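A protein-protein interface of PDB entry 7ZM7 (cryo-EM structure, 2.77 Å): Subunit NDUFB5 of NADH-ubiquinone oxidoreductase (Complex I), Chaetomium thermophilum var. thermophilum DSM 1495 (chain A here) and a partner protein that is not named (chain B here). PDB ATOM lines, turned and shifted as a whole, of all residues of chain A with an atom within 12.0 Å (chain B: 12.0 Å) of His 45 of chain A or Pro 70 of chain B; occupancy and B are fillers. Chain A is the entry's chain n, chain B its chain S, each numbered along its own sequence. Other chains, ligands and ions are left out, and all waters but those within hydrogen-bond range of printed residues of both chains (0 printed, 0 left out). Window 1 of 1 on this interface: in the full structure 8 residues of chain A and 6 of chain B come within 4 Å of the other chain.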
ATOM      1  N   GLY A  44       4.214  -0.644  10.191  1.00  0.00           N
ATOM      2  CA  GLY A  44       3.536  -1.502   9.200  1.00  0.00           C
ATOM      3  C   GLY A  44       2.151  -1.906   9.666  1.00  0.00           C
ATOM      4  O   GLY A  44       1.667  -1.318  10.650  1.00  0.00           O
ATOM      5  N   HIS A  45       1.528  -2.872   8.984  1.00  0.00           N
ATOM      6  CA  HIS A  45       0.202  -3.371   9.421  1.00  0.00           C
ATOM      7  C   HIS A  45       0.317  -4.842   9.807  1.00  0.00           C
ATOM      8  O   HIS A  45       1.433  -5.379   9.711  1.00  0.00           O
ATOM      9  CB  HIS A  45      -0.837  -3.169   8.321  1.00  0.00           C
ATOM     10  CG  HIS A  45      -0.476  -3.848   7.044  1.00  0.00           C
ATOM     11  ND1 HIS A  45      -0.712  -5.188   6.829  1.00  0.00           N
ATOM     12  CD2 HIS A  45       0.108  -3.380   5.922  1.00  0.00           C
ATOM     13  CE1 HIS A  45      -0.278  -5.520   5.635  1.00  0.00           C
ATOM     14  NE2 HIS A  45       0.223  -4.429   5.057  1.00  0.00           N
ATOM     15  N   ASN A  46      -0.791  -5.453  10.226  1.00  0.00           N
ATOM     16  CA  ASN A  46      -0.822  -6.891  10.582  1.00  0.00           C
ATOM     17  C   ASN A  46      -2.132  -7.492  10.067  1.00  0.00           C
ATOM     18  O   ASN A  46      -2.730  -8.289  10.809  1.00  0.00           O
ATOM     19  CB  ASN A  46      -0.761  -7.084  12.094  1.00  0.00           C
ATOM     20  CG  ASN A  46       0.451  -6.437  12.730  1.00  0.00           C
ATOM     21  OD1 ASN A  46       1.575  -6.900  12.549  1.00  0.00           O
ATOM     22  ND2 ASN A  46       0.233  -5.368  13.477  1.00  0.00           N
ATOM     23  N   VAL A  47      -2.559  -7.018   8.911  1.00  0.00           N
ATOM     24  CA  VAL A  47      -3.746  -7.620   8.269  1.00  0.00           C
ATOM     25  C   VAL A  47      -3.139  -8.811   7.571  1.00  0.00           C
ATOM     26  O   VAL A  47      -2.209  -8.623   6.782  1.00  0.00           O
ATOM     27  CB  VAL A  47      -4.401  -6.672   7.258  1.00  0.00           C
ATOM     28  CG1 VAL A  47      -5.600  -7.316   6.581  1.00  0.00           C
ATOM     29  CG2 VAL A  47      -4.798  -5.361   7.915  1.00  0.00           C
ATOM     30  N   GLU A  48      -3.586  -9.999   7.939  1.00  0.00           N
ATOM     31  CA  GLU A  48      -2.953 -11.191   7.382  1.00  0.00           C
ATOM     32  C   GLU A  48      -3.883 -11.751   6.321  1.00  0.00           C
ATOM     33  O   GLU A  48      -5.002 -11.257   6.198  1.00  0.00           O
ATOM     34  CB  GLU A  48      -2.573 -12.094   8.539  1.00  0.00           C
ATOM     35  CG  GLU A  48      -1.427 -11.546   9.366  1.00  0.00           C
ATOM     36  CD  GLU A  48      -0.723 -12.567  10.241  1.00  0.00           C
ATOM     37  OE1 GLU A  48      -1.296 -13.654  10.462  1.00  0.00           O
ATOM     38  OE2 GLU A  48       0.403 -12.279  10.689  1.00  0.00           O
ATOM     39  N   GLU A  49      -3.405 -12.717   5.549  1.00  0.00           N
ATOM     40  CA  GLU A  49      -4.197 -13.293   4.437  1.00  0.00           C
ATOM     41  C   GLU A  49      -4.229 -14.803   4.602  1.00  0.00           C
ATOM     42  O   GLU A  49      -3.161 -15.407   4.626  1.00  0.00           O
ATOM     43  CB  GLU A  49      -3.525 -12.988   3.096  1.00  0.00           C
ATOM     44  CG  GLU A  49      -4.070 -11.761   2.407  1.00  0.00           C
ATOM     45  CD  GLU A  49      -5.463 -11.933   1.836  1.00  0.00           C
ATOM     46  OE1 GLU A  49      -5.705 -12.960   1.181  1.00  0.00           O
ATOM     47  OE2 GLU A  49      -6.302 -11.044   2.062  1.00  0.00           O
ATOM     48  N   PRO A  50      -5.399 -15.444   4.716  1.00  0.00           N
ATOM     49  CA  PRO A  50      -5.431 -16.899   4.723  1.00  0.00           C
ATOM     50  C   PRO A  50      -5.126 -17.377   3.298  1.00  0.00           C
ATOM     51  O   PRO A  50      -5.574 -16.739   2.413  1.00  0.00           O
ATOM     52  CB  PRO A  50      -6.867 -17.205   5.168  1.00  0.00           C
ATOM     53  CG  PRO A  50      -7.666 -15.974   4.787  1.00  0.00           C
ATOM     54  CD  PRO A  50      -6.702 -14.811   4.886  1.00  0.00           C
ATOM     55  N   GLN B  67       5.960   1.989   1.479  1.00  0.00           N
ATOM     56  CA  GLN B  67       5.464   0.961   2.385  1.00  0.00           C
ATOM     57  C   GLN B  67       4.127   0.407   1.931  1.00  0.00           C
ATOM     58  O   GLN B  67       3.169   1.137   1.723  1.00  0.00           O
ATOM     59  CB  GLN B  67       5.344   1.511   3.806  1.00  0.00           C
ATOM     60  CG  GLN B  67       6.665   1.941   4.404  1.00  0.00           C
ATOM     61  CD  GLN B  67       6.568   2.189   5.893  1.00  0.00           C
ATOM     62  OE1 GLN B  67       5.493   2.079   6.481  1.00  0.00           O
ATOM     63  NE2 GLN B  67       7.693   2.525   6.510  1.00  0.00           N
ATOM     64  N   TYR B  68       4.078  -0.911   1.823  1.00  0.00           N
ATOM     65  CA  TYR B  68       2.900  -1.612   1.280  1.00  0.00           C
ATOM     66  C   TYR B  68       1.652  -1.490   2.146  1.00  0.00           C
ATOM     67  O   TYR B  68       1.749  -1.587   3.377  1.00  0.00           O
ATOM     68  CB  TYR B  68       3.329  -3.054   1.032  1.00  0.00           C
ATOM     69  CG  TYR B  68       4.427  -3.172   0.009  1.00  0.00           C
ATOM     70  CD1 TYR B  68       4.307  -2.570  -1.230  1.00  0.00           C
ATOM     71  CD2 TYR B  68       5.591  -3.864   0.283  1.00  0.00           C
ATOM     72  CE1 TYR B  68       5.315  -2.661  -2.174  1.00  0.00           C
ATOM     73  CE2 TYR B  68       6.605  -3.971  -0.652  1.00  0.00           C
ATOM     74  CZ  TYR B  68       6.465  -3.368  -1.885  1.00  0.00           C
ATOM     75  OH  TYR B  68       7.460  -3.459  -2.811  1.00  0.00           O
ATOM     76  N   ASP B  69       0.508  -1.299   1.504  1.00  0.00           N
ATOM     77  CA  ASP B  69      -0.791  -1.184   2.194  1.00  0.00           C
ATOM     78  C   ASP B  69      -1.342  -2.569   2.552  1.00  0.00           C
ATOM     79  O   ASP B  69      -0.888  -3.561   1.981  1.00  0.00           O
ATOM     80  CB  ASP B  69      -1.756  -0.464   1.266  1.00  0.00           C
ATOM     81  CG  ASP B  69      -1.606   1.044   1.306  1.00  0.00           C
ATOM     82  OD1 ASP B  69      -0.999   1.537   2.277  1.00  0.00           O
ATOM     83  OD2 ASP B  69      -2.095   1.712   0.372  1.00  0.00           O
ATOM     84  N   PRO B  70      -2.301  -2.685   3.496  1.00  0.00           N
ATOM     85  CA  PRO B  70      -2.934  -3.974   3.794  1.00  0.00           C
ATOM     86  C   PRO B  70      -3.814  -4.540   2.668  1.00  0.00           C
ATOM     87  O   PRO B  70      -4.345  -3.769   1.878  1.00  0.00           O
ATOM     88  CB  PRO B  70      -3.879  -3.546   4.905  1.00  0.00           C
ATOM     89  CG  PRO B  70      -4.167  -2.102   4.646  1.00  0.00           C
ATOM     90  CD  PRO B  70      -2.793  -1.586   4.320  1.00  0.00           C
ATOM     91  N   PRO B  71      -4.037  -5.864   2.571  1.00  0.00           N
ATOM     92  CA  PRO B  71      -4.788  -6.414   1.447  1.00  0.00           C
ATOM     93  C   PRO B  71      -6.253  -6.166   1.764  1.00  0.00           C
ATOM     94  O   PRO B  71      -6.559  -6.064   2.928  1.00  0.00           O
ATOM     95  CB  PRO B  71      -4.414  -7.900   1.446  1.00  0.00           C
ATOM     96  CG  PRO B  71      -3.289  -8.033   2.451  1.00  0.00           C
ATOM     97  CD  PRO B  71      -3.488  -6.903   3.436  1.00  0.00           C
ATOM     98  N   THR B  72      -7.117  -6.047   0.753  1.00  0.00           N
ATOM     99  CA  THR B  72      -8.466  -5.631   1.088  1.00  0.00           C
ATOM    100  C   THR B  72      -9.422  -6.226   0.067  1.00  0.00           C
ATOM    101  O   THR B  72      -9.050  -7.095  -0.723  1.00  0.00           O
ATOM    102  CB  THR B  72      -8.549  -4.100   1.161  1.00  0.00           C
ATOM    103  OG1 THR B  72      -9.801  -3.707   1.734  1.00  0.00           O
ATOM    104  CG2 THR B  72      -8.397  -3.477  -0.219  1.00  0.00           C
ATOM    105  N   GLY B  73     -10.664  -5.757   0.090  1.00  0.00           N
ATOM    106  CA  GLY B  73     -11.604  -6.170  -0.961  1.00  0.00           C
ATOM    107  C   GLY B  73     -12.804  -6.900  -0.435  1.00  0.00           C
ATOM    108  O   GLY B  73     -12.670  -7.626   0.551  1.00  0.00           O
ATOM    109  N   TRP B  74     -13.948  -6.705  -1.075  1.00  0.00           N
ATOM    110  CA  TRP B  74     -15.113  -7.528  -0.696  1.00  0.00           C
ATOM    111  C   TRP B  74     -15.211  -8.643  -1.729  1.00  0.00           C
ATOM    112  O   TRP B  74     -15.648  -8.359  -2.850  1.00  0.00           O
ATOM    113  CB  TRP B  74     -16.380  -6.685  -0.649  1.00  0.00           C
ATOM    114  CG  TRP B  74     -16.270  -5.490   0.244  1.00  0.00           C
ATOM    115  CD1 TRP B  74     -15.332  -5.265   1.207  1.00  0.00           C
ATOM    116  CD2 TRP B  74     -17.136  -4.344   0.251  1.00  0.00           C
ATOM    117  NE1 TRP B  74     -15.550  -4.057   1.807  1.00  0.00           N
ATOM    118  CE2 TRP B  74     -16.652  -3.472   1.246  1.00  0.00           C
ATOM    119  CE3 TRP B  74     -18.268  -3.976  -0.481  1.00  0.00           C
ATOM    120  CZ2 TRP B  74     -17.264  -2.254   1.524  1.00  0.00           C
ATOM    121  CZ3 TRP B  74     -18.871  -2.771  -0.206  1.00  0.00           C
ATOM    122  CH2 TRP B  74     -18.375  -1.926   0.784  1.00  0.00           C
ATOM    123  N   PRO B  80     -17.062  -6.837   5.279  1.00  0.00           N
ATOM    124  CA  PRO B  80     -16.349  -7.608   6.312  1.00  0.00           C
ATOM    125  C   PRO B  80     -17.207  -8.008   7.500  1.00  0.00           C
ATOM    126  O   PRO B  80     -16.829  -8.934   8.228  1.00  0.00           O
ATOM    127  CB  PRO B  80     -15.217  -6.663   6.737  1.00  0.00           C
ATOM    128  CG  PRO B  80     -15.668  -5.310   6.313  1.00  0.00           C
ATOM    129  CD  PRO B  80     -16.432  -5.527   5.052  1.00  0.00           C
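A ring nitrogen (NE2) of His 45 of chain A is in hydrogen-bond range of the backbone carbonyl oxygen of Asp 69 of chain B. A ring nitrogen (NE2) of His 45 of chain A sits close to the backbone nitrogen (N) of Pro 70 of chain B, at 3.4 Å.
Of the 7 printed residues of chain A, 3 touch a printed residue of chain B. Printed residues of chain A that touch a printed residue of chain B: His 45, Val 47 and Glu 49. Of the 9 printed residues of chain B, 4 touch a printed residue of chain A. Along chain B the printed residues that touch a printed residue of chain A span positions 68 to 71. Among the printed residues, 6 pairs touch across the chains. Among the printed residues, no Asp or Glu carboxylate lies within 4 Å of a Lys or Arg side-chain nitrogen of the other chain.
Of chain B, only Tyr 68 (3.5 Å), Asp 69 (3.4 Å) and Pro 70 (3.4 Å) come within 4 Å of His 45 of chain A. Pro 70 of chain B touches just these residues of chain A: His 45 and Val 47. No residue of chain B comes within 4 Å of Asn 46 of chain A. Asp 69 of chain B touches just one residue of chain A: His 45. Pro 71 of chain B touches two residues of chain A. No residue of chain A comes within 4 Å of Thr 72 of chain B. Of the printed residues of chain A, Tyr 68 of chain B touches His 45. Of the printed residues of chain B, Glu 49 of chain A touches Pro 71 (3.7 Å). Glu 48 of chain A touches none of the printed residues of chain B. The nearest residue of chain A that does not touch Pro 70 of chain B is Asn 46 of chain A (6.4 Å). The nearest printed residue of chain A that does not touch Tyr 68 of chain B is Gly 44 of chain A (6.1 Å).
CD2 of His 45 of chain A touches O of Tyr 68 of chain B, 3.5 Å away. Val 47 of chain A touches Pro 70 of chain B. Val 47 of chain A touches Pro 71 of chain B (CG1 to CD, 3.8 Å). Pro 71 of chain B touches Glu 49 of chain A (CB to OE2, 3.7 Å).
A ring nitrogen (ND1) of His 45 of chain A sits at hydrogen-bond distance from the backbone NH (N) of Val 47 of chain A, 3.3 Å away.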
